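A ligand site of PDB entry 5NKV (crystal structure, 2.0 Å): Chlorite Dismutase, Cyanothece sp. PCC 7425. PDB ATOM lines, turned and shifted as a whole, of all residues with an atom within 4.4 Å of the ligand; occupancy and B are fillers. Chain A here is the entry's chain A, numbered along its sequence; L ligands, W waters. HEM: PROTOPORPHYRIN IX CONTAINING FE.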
ATOM      1  N   ASN A  64      -0.593 -25.604   7.239  1.00  0.00           N
ATOM      2  CA  ASN A  64      -1.654 -25.820   8.207  1.00  0.00           C
ATOM      3  C   ASN A  64      -1.095 -26.383   9.500  1.00  0.00           C
ATOM      4  O   ASN A  64       0.037 -26.880   9.571  1.00  0.00           O
ATOM      5  CB  ASN A  64      -2.706 -26.768   7.642  1.00  0.00           C
ATOM      6  CG  ASN A  64      -2.107 -28.098   7.195  1.00  0.00           C
ATOM      7  OD1 ASN A  64      -1.474 -28.190   6.153  1.00  0.00           O
ATOM      8  ND2 ASN A  64      -2.301 -29.134   8.007  1.00  0.00           N
ATOM      9  N   ILE A  65      -1.914 -26.293  10.550  1.00  0.00           N
ATOM     10  CA  ILE A  65      -1.568 -26.867  11.844  1.00  0.00           C
ATOM     11  C   ILE A  65      -1.376 -28.371  11.707  1.00  0.00           C
ATOM     12  O   ILE A  65      -2.154 -29.061  11.033  1.00  0.00           O
ATOM     13  CB  ILE A  65      -2.658 -26.526  12.875  1.00  0.00           C
ATOM     14  CG1 ILE A  65      -2.719 -25.017  13.125  1.00  0.00           C
ATOM     15  CG2 ILE A  65      -2.445 -27.283  14.194  1.00  0.00           C
ATOM     16  CD1 ILE A  65      -1.467 -24.433  13.763  1.00  0.00           C
ATOM     17  N   ARG A  66      -0.333 -28.885  12.364  1.00  0.00           N
ATOM     18  CA  ARG A  66      -0.011 -30.301  12.315  1.00  0.00           C
ATOM     19  C   ARG A  66      -0.203 -31.021  13.650  1.00  0.00           C
ATOM     20  O   ARG A  66      -0.373 -32.239  13.646  1.00  0.00           O
ATOM     21  CB  ARG A  66       1.450 -30.505  11.866  1.00  0.00           C
ATOM     22  CG  ARG A  66       1.827 -29.748  10.602  1.00  0.00           C
ATOM     23  CD  ARG A  66       1.022 -30.199   9.395  1.00  0.00           C
ATOM     24  NE  ARG A  66       1.413 -29.474   8.186  1.00  0.00           N
ATOM     25  CZ  ARG A  66       2.400 -29.851   7.378  1.00  0.00           C
ATOM     26  NH1 ARG A  66       3.105 -30.944   7.609  1.00  0.00           N
ATOM     27  NH2 ARG A  66       2.675 -29.121   6.304  1.00  0.00           N
ATOM     28  N   TYR A  67      -0.182 -30.295  14.775  1.00  0.00           N
ATOM     29  CA  TYR A  67      -0.206 -30.953  16.084  1.00  0.00           C
ATOM     30  C   TYR A  67      -1.157 -30.273  17.068  1.00  0.00           C
ATOM     31  O   TYR A  67      -1.828 -30.946  17.849  1.00  0.00           O
ATOM     32  CB  TYR A  67       1.196 -30.994  16.682  1.00  0.00           C
ATOM     33  CG  TYR A  67       2.149 -31.887  15.920  1.00  0.00           C
ATOM     34  CD1 TYR A  67       2.031 -33.265  15.980  1.00  0.00           C
ATOM     35  CD2 TYR A  67       3.178 -31.352  15.147  1.00  0.00           C
ATOM     36  CE1 TYR A  67       2.899 -34.092  15.288  1.00  0.00           C
ATOM     37  CE2 TYR A  67       4.054 -32.168  14.453  1.00  0.00           C
ATOM     38  CZ  TYR A  67       3.910 -33.544  14.525  1.00  0.00           C
ATOM     39  OH  TYR A  67       4.765 -34.369  13.839  1.00  0.00           O
ATOM     40  N   ALA A  68      -1.223 -28.947  17.030  1.00  0.00           N
ATOM     41  CA  ALA A  68      -1.990 -28.213  18.043  1.00  0.00           C
ATOM     42  C   ALA A  68      -3.469 -28.588  17.997  1.00  0.00           C
ATOM     43  O   ALA A  68      -4.056 -28.716  16.917  1.00  0.00           O
ATOM     44  CB  ALA A  68      -1.822 -26.717  17.844  1.00  0.00           C
ATOM     45  N   LEU A  76      -3.075 -19.950  22.519  1.00  0.00           N
ATOM     46  CA  LEU A  76      -2.052 -19.258  21.731  1.00  0.00           C
ATOM     47  C   LEU A  76      -2.620 -17.988  21.115  1.00  0.00           C
ATOM     48  O   LEU A  76      -2.007 -16.913  21.210  1.00  0.00           O
ATOM     49  CB  LEU A  76      -1.521 -20.188  20.643  1.00  0.00           C
ATOM     50  CG  LEU A  76      -0.542 -21.264  21.120  1.00  0.00           C
ATOM     51  CD1 LEU A  76      -0.471 -22.408  20.121  1.00  0.00           C
ATOM     52  CD2 LEU A  76       0.838 -20.656  21.321  1.00  0.00           C
ATOM     53  N   ILE A  94      16.124 -19.814  13.351  1.00  0.00           N
ATOM     54  CA  ILE A  94      16.684 -21.093  13.785  1.00  0.00           C
ATOM     55  C   ILE A  94      16.256 -22.195  12.814  1.00  0.00           C
ATOM     56  O   ILE A  94      15.157 -22.753  12.954  1.00  0.00           O
ATOM     57  CB  ILE A  94      16.251 -21.425  15.220  1.00  0.00           C
ATOM     58  CG1 ILE A  94      16.688 -20.317  16.175  1.00  0.00           C
ATOM     59  CG2 ILE A  94      16.859 -22.764  15.652  1.00  0.00           C
ATOM     60  CD1 ILE A  94      16.232 -20.510  17.614  1.00  0.00           C
ATOM     61  N   ILE A  96      16.109 -25.942  11.583  1.00  0.00           N
ATOM     62  CA  ILE A  96      16.113 -27.186  12.344  1.00  0.00           C
ATOM     63  C   ILE A  96      15.867 -28.355  11.392  1.00  0.00           C
ATOM     64  O   ILE A  96      15.071 -28.240  10.447  1.00  0.00           O
ATOM     65  CB  ILE A  96      15.063 -27.165  13.468  1.00  0.00           C
ATOM     66  CG1 ILE A  96      15.533 -26.239  14.602  1.00  0.00           C
ATOM     67  CG2 ILE A  96      14.798 -28.579  14.012  1.00  0.00           C
ATOM     68  CD1 ILE A  96      14.469 -25.951  15.635  1.00  0.00           C
ATOM     69  N   LYS A  98      15.157 -32.679  11.742  1.00  0.00           N
ATOM     70  CA  LYS A  98      14.912 -33.817  12.601  1.00  0.00           C
ATOM     71  C   LYS A  98      15.334 -35.108  11.900  1.00  0.00           C
ATOM     72  O   LYS A  98      15.406 -35.171  10.671  1.00  0.00           O
ATOM     73  CB  LYS A  98      13.441 -33.895  13.010  1.00  0.00           C
ATOM     74  CG  LYS A  98      12.999 -32.748  13.905  1.00  0.00           C
ATOM     75  CD  LYS A  98      11.590 -32.957  14.460  1.00  0.00           C
ATOM     76  CE  LYS A  98      11.175 -31.814  15.380  1.00  0.00           C
ATOM     77  NZ  LYS A  98       9.875 -32.073  16.046  1.00  0.00           N
ATOM     78  N   TRP A 102      12.314 -39.809  13.315  1.00  0.00           N
ATOM     79  CA  TRP A 102      11.167 -38.986  13.676  1.00  0.00           C
ATOM     80  C   TRP A 102      10.098 -39.039  12.587  1.00  0.00           C
ATOM     81  O   TRP A 102       8.901 -39.208  12.882  1.00  0.00           O
ATOM     82  CB  TRP A 102      11.610 -37.546  13.913  1.00  0.00           C
ATOM     83  CG  TRP A 102      10.473 -36.564  14.008  1.00  0.00           C
ATOM     84  CD1 TRP A 102       9.951 -35.805  13.002  1.00  0.00           C
ATOM     85  CD2 TRP A 102       9.725 -36.249  15.192  1.00  0.00           C
ATOM     86  NE1 TRP A 102       8.925 -35.030  13.481  1.00  0.00           N
ATOM     87  CE2 TRP A 102       8.761 -35.280  14.820  1.00  0.00           C
ATOM     88  CE3 TRP A 102       9.764 -36.684  16.518  1.00  0.00           C
ATOM     89  CZ2 TRP A 102       7.855 -34.752  15.732  1.00  0.00           C
ATOM     90  CZ3 TRP A 102       8.862 -36.152  17.422  1.00  0.00           C
ATOM     91  CH2 TRP A 102       7.921 -35.197  17.018  1.00  0.00           C
ATOM     92  N   PHE A 114       5.717 -34.676  21.170  1.00  0.00           N
ATOM     93  CA  PHE A 114       5.730 -33.227  20.987  1.00  0.00           C
ATOM     94  C   PHE A 114       5.202 -32.504  22.214  1.00  0.00           C
ATOM     95  O   PHE A 114       5.822 -31.546  22.703  1.00  0.00           O
ATOM     96  CB  PHE A 114       4.918 -32.854  19.747  1.00  0.00           C
ATOM     97  CG  PHE A 114       4.801 -31.376  19.530  1.00  0.00           C
ATOM     98  CD1 PHE A 114       5.843 -30.653  18.978  1.00  0.00           C
ATOM     99  CD2 PHE A 114       3.637 -30.703  19.872  1.00  0.00           C
ATOM    100  CE1 PHE A 114       5.738 -29.284  18.777  1.00  0.00           C
ATOM    101  CE2 PHE A 114       3.528 -29.342  19.666  1.00  0.00           C
ATOM    102  CZ  PHE A 114       4.574 -28.628  19.124  1.00  0.00           C
ATOM    103  N   HIS A 120       5.898 -29.042  24.468  1.00  0.00           N
ATOM    104  CA  HIS A 120       6.419 -27.994  23.584  1.00  0.00           C
ATOM    105  C   HIS A 120       5.566 -26.737  23.670  1.00  0.00           C
ATOM    106  O   HIS A 120       6.087 -25.628  23.829  1.00  0.00           O
ATOM    107  CB  HIS A 120       6.478 -28.530  22.148  1.00  0.00           C
ATOM    108  CG  HIS A 120       7.245 -27.653  21.206  1.00  0.00           C
ATOM    109  ND1 HIS A 120       8.397 -28.077  20.580  1.00  0.00           N
ATOM    110  CD2 HIS A 120       7.024 -26.387  20.782  1.00  0.00           C
ATOM    111  CE1 HIS A 120       8.862 -27.112  19.810  1.00  0.00           C
ATOM    112  NE2 HIS A 120       8.046 -26.079  19.910  1.00  0.00           N
ATOM    113  N   THR A 121       4.246 -26.890  23.546  1.00  0.00           N
ATOM    114  CA  THR A 121       3.364 -25.725  23.523  1.00  0.00           C
ATOM    115  C   THR A 121       3.243 -25.097  24.906  1.00  0.00           C
ATOM    116  O   THR A 121       3.289 -23.869  25.044  1.00  0.00           O
ATOM    117  CB  THR A 121       1.980 -26.124  22.998  1.00  0.00           C
ATOM    118  OG1 THR A 121       2.130 -26.742  21.710  1.00  0.00           O
ATOM    119  CG2 THR A 121       1.078 -24.900  22.869  1.00  0.00           C
ATOM    120  N   GLY A 124       6.516 -23.209  25.750  1.00  0.00           N
ATOM    121  CA  GLY A 124       6.691 -21.995  24.975  1.00  0.00           C
ATOM    122  C   GLY A 124       5.643 -20.940  25.279  1.00  0.00           C
ATOM    123  O   GLY A 124       5.916 -19.739  25.171  1.00  0.00           O
ATOM    124  N   LEU A 125       4.444 -21.367  25.661  1.00  0.00           N
ATOM    125  CA  LEU A 125       3.353 -20.428  25.898  1.00  0.00           C
ATOM    126  C   LEU A 125       3.639 -19.506  27.077  1.00  0.00           C
ATOM    127  O   LEU A 125       3.015 -18.437  27.176  1.00  0.00           O
ATOM    128  CB  LEU A 125       2.052 -21.208  26.142  1.00  0.00           C
ATOM    129  CG  LEU A 125       0.741 -20.433  26.179  1.00  0.00           C
ATOM    130  CD1 LEU A 125       0.569 -19.554  24.953  1.00  0.00           C
ATOM    131  CD2 LEU A 125      -0.419 -21.412  26.284  1.00  0.00           C
ATOM    132  N   LEU A 128       5.302 -15.973  26.025  1.00  0.00           N
ATOM    133  CA  LEU A 128       4.494 -14.985  25.328  1.00  0.00           C
ATOM    134  C   LEU A 128       3.849 -14.039  26.336  1.00  0.00           C
ATOM    135  O   LEU A 128       3.627 -14.420  27.493  1.00  0.00           O
ATOM    136  CB  LEU A 128       3.403 -15.660  24.500  1.00  0.00           C
ATOM    137  CG  LEU A 128       3.821 -16.193  23.129  1.00  0.00           C
ATOM    138  CD1 LEU A 128       5.063 -17.053  23.199  1.00  0.00           C
ATOM    139  CD2 LEU A 128       2.678 -16.964  22.500  1.00  0.00           C
ATOM    140  N   VAL A 131       7.741 -13.100  23.121  1.00  0.00           N
ATOM    141  CA  VAL A 131       8.309 -13.609  21.882  1.00  0.00           C
ATOM    142  C   VAL A 131       7.191 -13.786  20.867  1.00  0.00           C
ATOM    143  O   VAL A 131       6.208 -14.491  21.139  1.00  0.00           O
ATOM    144  CB  VAL A 131       9.066 -14.931  22.107  1.00  0.00           C
ATOM    145  CG1 VAL A 131       9.611 -15.468  20.793  1.00  0.00           C
ATOM    146  CG2 VAL A 131      10.183 -14.737  23.117  1.00  0.00           C
ATOM    147  N   ARG A 133       6.448 -15.347  17.001  1.00  0.00           N
ATOM    148  CA  ARG A 133       7.005 -16.520  16.344  1.00  0.00           C
ATOM    149  C   ARG A 133       6.347 -16.754  15.000  1.00  0.00           C
ATOM    150  O   ARG A 133       5.182 -16.405  14.792  1.00  0.00           O
ATOM    151  CB  ARG A 133       6.866 -17.771  17.220  1.00  0.00           C
ATOM    152  CG  ARG A 133       5.454 -18.329  17.261  1.00  0.00           C
ATOM    153  CD  ARG A 133       5.345 -19.492  18.234  1.00  0.00           C
ATOM    154  NE  ARG A 133       4.154 -20.285  17.975  1.00  0.00           N
ATOM    155  CZ  ARG A 133       2.910 -19.903  18.296  1.00  0.00           C
ATOM    156  NH1 ARG A 133       2.710 -18.729  18.879  1.00  0.00           N
ATOM    157  NH2 ARG A 133       1.883 -20.691  18.021  1.00  0.00           N
ATOM    158  N   LEU A 135       6.495 -20.113  11.975  1.00  0.00           N
ATOM    159  CA  LEU A 135       6.960 -21.454  11.645  1.00  0.00           C
ATOM    160  C   LEU A 135       6.820 -21.676  10.149  1.00  0.00           C
ATOM    161  O   LEU A 135       5.735 -21.461   9.587  1.00  0.00           O
ATOM    162  CB  LEU A 135       6.172 -22.511  12.415  1.00  0.00           C
ATOM    163  CG  LEU A 135       6.464 -23.971  12.045  1.00  0.00           C
ATOM    164  CD1 LEU A 135       7.896 -24.331  12.359  1.00  0.00           C
ATOM    165  CD2 LEU A 135       5.495 -24.901  12.749  1.00  0.00           C
ATOM    166  N   PHE A 147      12.650 -27.328   9.028  1.00  0.00           N
ATOM    167  CA  PHE A 147      11.852 -26.188   9.461  1.00  0.00           C
ATOM    168  C   PHE A 147      12.729 -24.939   9.515  1.00  0.00           C
ATOM    169  O   PHE A 147      13.921 -25.002   9.799  1.00  0.00           O
ATOM    170  CB  PHE A 147      11.237 -26.406  10.849  1.00  0.00           C
ATOM    171  CG  PHE A 147      10.494 -27.704  10.997  1.00  0.00           C
ATOM    172  CD1 PHE A 147       9.177 -27.818  10.583  1.00  0.00           C
ATOM    173  CD2 PHE A 147      11.102 -28.808  11.578  1.00  0.00           C
ATOM    174  CE1 PHE A 147       8.491 -29.007  10.727  1.00  0.00           C
ATOM    175  CE2 PHE A 147      10.417 -29.997  11.722  1.00  0.00           C
ATOM    176  CZ  PHE A 147       9.111 -30.097  11.297  1.00  0.00           C
ATOM    177  N   THR A 149      12.337 -21.612  11.769  1.00  0.00           N
ATOM    178  CA  THR A 149      11.610 -20.975  12.857  1.00  0.00           C
ATOM    179  C   THR A 149      12.136 -19.559  13.041  1.00  0.00           C
ATOM    180  O   THR A 149      13.346 -19.313  12.976  1.00  0.00           O
ATOM    181  CB  THR A 149      11.744 -21.767  14.165  1.00  0.00           C
ATOM    182  OG1 THR A 149      13.118 -21.798  14.567  1.00  0.00           O
ATOM    183  CG2 THR A 149      11.247 -23.194  13.980  1.00  0.00           C
ATOM    184  N   PHE A 151      11.740 -15.901  15.365  1.00  0.00           N
ATOM    185  CA  PHE A 151      11.302 -15.280  16.606  1.00  0.00           C
ATOM    186  C   PHE A 151      11.820 -13.855  16.655  1.00  0.00           C
ATOM    187  O   PHE A 151      12.948 -13.582  16.221  1.00  0.00           O
ATOM    188  CB  PHE A 151      11.797 -16.067  17.832  1.00  0.00           C
ATOM    189  CG  PHE A 151      11.538 -17.539  17.745  1.00  0.00           C
ATOM    190  CD1 PHE A 151      10.350 -18.069  18.208  1.00  0.00           C
ATOM    191  CD2 PHE A 151      12.475 -18.391  17.191  1.00  0.00           C
ATOM    192  CE1 PHE A 151      10.098 -19.430  18.127  1.00  0.00           C
ATOM    193  CE2 PHE A 151      12.240 -19.750  17.096  1.00  0.00           C
ATOM    194  CZ  PHE A 151      11.047 -20.267  17.563  1.00  0.00           C
ATOM    195  N   PHE A 161      14.398 -15.451  26.307  1.00  0.00           N
ATOM    196  CA  PHE A 161      14.412 -16.302  25.118  1.00  0.00           C
ATOM    197  C   PHE A 161      15.551 -17.310  25.184  1.00  0.00           C
ATOM    198  O   PHE A 161      15.379 -18.484  24.829  1.00  0.00           O
ATOM    199  CB  PHE A 161      14.535 -15.449  23.857  1.00  0.00           C
ATOM    200  CG  PHE A 161      14.516 -16.252  22.586  1.00  0.00           C
ATOM    201  CD1 PHE A 161      13.320 -16.720  22.059  1.00  0.00           C
ATOM    202  CD2 PHE A 161      15.693 -16.537  21.915  1.00  0.00           C
ATOM    203  CE1 PHE A 161      13.295 -17.452  20.892  1.00  0.00           C
ATOM    204  CE2 PHE A 161      15.676 -17.275  20.750  1.00  0.00           C
ATOM    205  CZ  PHE A 161      14.479 -17.738  20.237  1.00  0.00           C
ATOM    206  N   LEU A 164      14.465 -20.163  27.338  1.00  0.00           N
ATOM    207  CA  LEU A 164      13.565 -21.067  26.619  1.00  0.00           C
ATOM    208  C   LEU A 164      14.344 -22.059  25.775  1.00  0.00           C
ATOM    209  O   LEU A 164      14.028 -23.254  25.738  1.00  0.00           O
ATOM    210  CB  LEU A 164      12.613 -20.244  25.751  1.00  0.00           C
ATOM    211  CG  LEU A 164      11.754 -21.021  24.756  1.00  0.00           C
ATOM    212  CD1 LEU A 164      10.784 -21.947  25.474  1.00  0.00           C
ATOM    213  CD2 LEU A 164      11.006 -20.054  23.871  1.00  0.00           C
ATOM    214  N   LEU A 165      15.380 -21.585  25.064  1.00  0.00           N
ATOM    215  CA  LEU A 165      16.159 -22.466  24.211  1.00  0.00           C
ATOM    216  C   LEU A 165      16.804 -23.588  25.027  1.00  0.00           C
ATOM    217  O   LEU A 165      16.762 -24.763  24.631  1.00  0.00           O
ATOM    218  CB  LEU A 165      17.224 -21.674  23.457  1.00  0.00           C
ATOM    219  CG  LEU A 165      16.735 -20.599  22.483  1.00  0.00           C
ATOM    220  CD1 LEU A 165      17.920 -19.867  21.866  1.00  0.00           C
ATOM    221  CD2 LEU A 165      15.862 -21.203  21.402  1.00  0.00           C
ATOM    222  N   MET A 168      13.954 -26.093  25.871  1.00  0.00           N
ATOM    223  CA  MET A 168      13.504 -26.894  24.733  1.00  0.00           C
ATOM    224  C   MET A 168      14.545 -27.937  24.345  1.00  0.00           C
ATOM    225  O   MET A 168      14.201 -29.092  24.088  1.00  0.00           O
ATOM    226  CB  MET A 168      13.205 -25.971  23.544  1.00  0.00           C
ATOM    227  CG  MET A 168      12.049 -26.453  22.685  1.00  0.00           C
ATOM    228  SD  MET A 168      10.442 -25.929  23.306  1.00  0.00           S
ATOM    229  CE  MET A 168      10.480 -24.195  22.875  1.00  0.00           C
ATOM    230  N   GLU A 173      11.710 -34.184  22.688  1.00  0.00           N
ATOM    231  CA  GLU A 173      11.614 -33.862  21.264  1.00  0.00           C
ATOM    232  C   GLU A 173      12.976 -33.616  20.651  1.00  0.00           C
ATOM    233  O   GLU A 173      13.245 -34.036  19.524  1.00  0.00           O
ATOM    234  CB  GLU A 173      10.716 -32.640  21.061  1.00  0.00           C
ATOM    235  CG  GLU A 173      10.518 -32.251  19.588  1.00  0.00           C
ATOM    236  CD  GLU A 173       9.777 -30.934  19.431  1.00  0.00           C
ATOM    237  OE1 GLU A 173       9.512 -30.278  20.463  1.00  0.00           O
ATOM    238  OE2 GLU A 173       9.463 -30.558  18.283  1.00  0.00           O
ATOM    239  N   TRP A 174      13.866 -32.938  21.381  1.00  0.00           N
ATOM    240  CA  TRP A 174      15.149 -32.548  20.817  1.00  0.00           C
ATOM    241  C   TRP A 174      16.120 -33.710  20.692  1.00  0.00           C
ATOM    242  O   TRP A 174      17.201 -33.534  20.112  1.00  0.00           O
ATOM    243  CB  TRP A 174      15.775 -31.424  21.636  1.00  0.00           C
ATOM    244  CG  TRP A 174      15.853 -30.153  20.859  1.00  0.00           C
ATOM    245  CD1 TRP A 174      16.988 -29.571  20.355  1.00  0.00           C
ATOM    246  CD2 TRP A 174      14.764 -29.310  20.482  1.00  0.00           C
ATOM    247  NE1 TRP A 174      16.662 -28.415  19.695  1.00  0.00           N
ATOM    248  CE2 TRP A 174      15.302 -28.228  19.759  1.00  0.00           C
ATOM    249  CE3 TRP A 174      13.383 -29.363  20.693  1.00  0.00           C
ATOM    250  CZ2 TRP A 174      14.514 -27.214  19.234  1.00  0.00           C
ATOM    251  CZ3 TRP A 174      12.596 -28.350  20.168  1.00  0.00           C
ATOM    252  CH2 TRP A 174      13.162 -27.292  19.461  1.00  0.00           C
ATOM    253  N   GLU A 180      20.932 -27.960  13.884  1.00  0.00           N
ATOM    254  CA  GLU A 180      20.338 -26.749  14.402  1.00  0.00           C
ATOM    255  C   GLU A 180      21.364 -25.616  14.346  1.00  0.00           C
ATOM    256  O   GLU A 180      22.539 -25.826  14.663  1.00  0.00           O
ATOM    257  CB  GLU A 180      19.842 -26.950  15.839  1.00  0.00           C
ATOM    258  CG  GLU A 180      19.120 -25.742  16.421  1.00  0.00           C
ATOM    259  CD  GLU A 180      18.551 -26.030  17.789  1.00  0.00           C
ATOM    260  OE1 GLU A 180      18.778 -27.149  18.313  1.00  0.00           O
ATOM    261  OE2 GLU A 180      17.873 -25.144  18.354  1.00  0.00           O
HETATM  262  CHA HEM L   1       6.095 -26.255  16.315  1.00  0.00           C
HETATM  263  CHB HEM L   1       4.539 -23.247  19.779  1.00  0.00           C
HETATM  264  CHC HEM L   1       9.126 -21.857  20.547  1.00  0.00           C
HETATM  265  CHD HEM L   1      10.699 -25.011  17.221  1.00  0.00           C
HETATM  266  C1A HEM L   1       5.270 -25.588  17.203  1.00  0.00           C
HETATM  267  C2A HEM L   1       3.839 -25.786  17.354  1.00  0.00           C
HETATM  268  C3A HEM L   1       3.419 -24.960  18.319  1.00  0.00           C
HETATM  269  C4A HEM L   1       4.552 -24.208  18.798  1.00  0.00           C
HETATM  270  CMA HEM L   1       1.965 -24.821  18.816  1.00  0.00           C
HETATM  271  CAA HEM L   1       2.959 -26.781  16.567  1.00  0.00           C
HETATM  272  CBA HEM L   1       2.564 -26.211  15.218  1.00  0.00           C
HETATM  273  CGA HEM L   1       1.588 -27.141  14.544  1.00  0.00           C
HETATM  274  O1A HEM L   1       1.665 -27.298  13.298  1.00  0.00           O
HETATM  275  O2A HEM L   1       0.726 -27.726  15.249  1.00  0.00           O
HETATM  276  C1B HEM L   1       5.639 -22.539  20.231  1.00  0.00           C
HETATM  277  C2B HEM L   1       5.601 -21.365  21.078  1.00  0.00           C
HETATM  278  C3B HEM L   1       6.855 -20.956  21.287  1.00  0.00           C
HETATM  279  C4B HEM L   1       7.748 -21.880  20.588  1.00  0.00           C
HETATM  280  CMB HEM L   1       4.299 -20.706  21.596  1.00  0.00           C
HETATM  281  CAB HEM L   1       7.206 -19.714  22.146  1.00  0.00           C
HETATM  282  CBB HEM L   1       8.430 -19.190  22.232  1.00  0.00           C
HETATM  283  C1C HEM L   1       9.941 -22.620  19.745  1.00  0.00           C
HETATM  284  C2C HEM L   1      11.397 -22.600  19.770  1.00  0.00           C
HETATM  285  C3C HEM L   1      11.848 -23.472  18.851  1.00  0.00           C
HETATM  286  C4C HEM L   1      10.678 -24.075  18.224  1.00  0.00           C
HETATM  287  CMC HEM L   1      12.163 -21.667  20.750  1.00  0.00           C
HETATM  288  CAC HEM L   1      13.281 -23.886  18.421  1.00  0.00           C
HETATM  289  CBC HEM L   1      14.425 -23.458  18.962  1.00  0.00           C
HETATM  290  C1D HEM L   1       9.589 -25.620  16.674  1.00  0.00           C
HETATM  291  C2D HEM L   1       9.576 -26.629  15.630  1.00  0.00           C
HETATM  292  C3D HEM L   1       8.313 -26.954  15.382  1.00  0.00           C
HETATM  293  C4D HEM L   1       7.468 -26.185  16.268  1.00  0.00           C
HETATM  294  CMD HEM L   1      10.841 -27.188  14.940  1.00  0.00           C
HETATM  295  CAD HEM L   1       7.805 -27.994  14.357  1.00  0.00           C
HETATM  296  CBD HEM L   1       7.973 -29.384  14.967  1.00  0.00           C
HETATM  297  CGD HEM L   1       7.365 -30.433  14.069  1.00  0.00           C
HETATM  298  O1D HEM L   1       7.845 -31.596  14.117  1.00  0.00           O
HETATM  299  O2D HEM L   1       6.412 -30.124  13.315  1.00  0.00           O
HETATM  300  NA  HEM L   1       5.672 -24.617  18.098  1.00  0.00           N
HETATM  301  NB  HEM L   1       6.954 -22.829  19.956  1.00  0.00           N
HETATM  302  NC  HEM L   1       9.545 -23.532  18.782  1.00  0.00           N
HETATM  303  ND  HEM L   1       8.279 -25.383  17.038  1.00  0.00           N
HETATM  304 FE   HEM L   1       7.602 -24.118  18.477  1.00  0.00          FE
HETATM  305  O   HOH W   1       4.714 -22.055  16.182  1.00  0.00           O
HETATM  306  O   HOH W   2       2.212 -25.825  11.007  1.00  0.00           O
HETATM  307  O   HOH W   3       4.495 -28.143  12.920  1.00  0.00           O
HETATM  308  O   HOH W   4       5.443 -31.455  10.795  1.00  0.00           O
HETATM  309  O   HOH W   5       6.777 -33.223  12.615  1.00  0.00           O
HETATM  310  O   HOH W   6       7.390 -22.331  16.707  1.00  0.00           O
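The backbone NH (N) of Tyr 67 is in hydrogen-bond range of an oxygen (O2A) of the ligand (2.8 Å).
The side-chain amino group (NZ) of Lys 98 lies within salt-bridge range of an oxygen (O1D) of the ligand (2.8 Å).
The backbone NH (N) of Ala 68 lies within hydrogen-bond range of an oxygen (O2A) of the ligand (2.9 Å).
A ring nitrogen (NE2) of His 120 binds an iron atom (FE) of the ligand, at 2.5 Å.
The backbone NH (N) of Arg 66 is in hydrogen-bond range of an oxygen (O1A) of the ligand, at 2.7 Å.
The indole nitrogen of Trp 174 is in hydrogen-bond range of the side-chain carboxylate of Glu 180.
The guanidinium group (NE) of Arg 66 sits at hydrogen-bond distance from the backbone carbonyl oxygen (O) of Asn 64 (3.2 Å).
The backbone NH (N) of His 120 sits at hydrogen-bond distance from the backbone carbonyl oxygen (O) of Phe 114.
A ring nitrogen (ND1) of His 120 lies within hydrogen-bond range of the side-chain carboxylate (OE1) of Glu 173 (2.5 Å).
O of Ile 96 is in hydrogen-bond range of N of Phe 147 (3.0 Å).
NZ of Lys 98 is in salt-bridge range of OE2 of Glu 173 (2.7 Å).
The backbone carbonyl oxygen (O) of Ile 94 sits at hydrogen-bond distance from the side-chain hydroxyl (OG1) of Thr 149 (2.8 Å).
Ile 65 touches the ligand (CG2 to O2A, 3.4 Å).
CD2 of Leu 76 touches CMB of the ligand, 3.5 Å away.
Ile 94 touches the ligand (CD1 to CBC, 3.7 Å).
Ile 96 touches the ligand.
Trp 102 touches the ligand (CZ2 to O1D, 3.5 Å).
Phe 114 touches the ligand (CZ to C2A, 3.4 Å).
OG1 of Thr 121 touches CMA of the ligand (3.5 Å).
Gly 124 touches the ligand.
Leu 128 touches the ligand.
Arg 133 touches the ligand (CD to C2B, 3.4 Å).
Leu 135 touches the ligand.
CZ of Phe 147 touches CGD of the ligand (3.3 Å).
CG2 of Thr 149 touches CHD of the ligand, 3.8 Å away.
CZ of Phe 151 touches C2C of the ligand, at 3.2 Å.
CD2 of Leu 164 touches CBB of the ligand, at 3.2 Å.
Leu 165 touches the ligand.
CE of Met 168 touches C1C of the ligand (3.5 Å).
Glu 173 touches the ligand (OE2 to CBD, 3.8 Å).
CH2 of Trp 174 touches CAC of the ligand, at 3.6 Å.
OE2 of Glu 180 touches CBC of the ligand (3.9 Å).
Hydrophobic or aromatic side chains within 4 Å of the ligand: Ile 65, Tyr 67, Ala 68, Leu 76, Ile 94, Ile 96, Trp 102, Phe 114, His 120, Leu 128, Leu 135, Phe 147, Phe 151, Leu 164, Leu 165, Met 168 and Trp 174.
Water W5 lies within hydrogen-bond range of O1D of the ligand (2.5 Å), OH of Tyr 67 (2.6 Å) and NE1 of Trp 102 (2.9 Å).
Water W2 bridges an oxygen (O1A) of the ligand (2.8 Å) and the backbone carbonyl oxygen of Asn 64 (2.8 Å).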
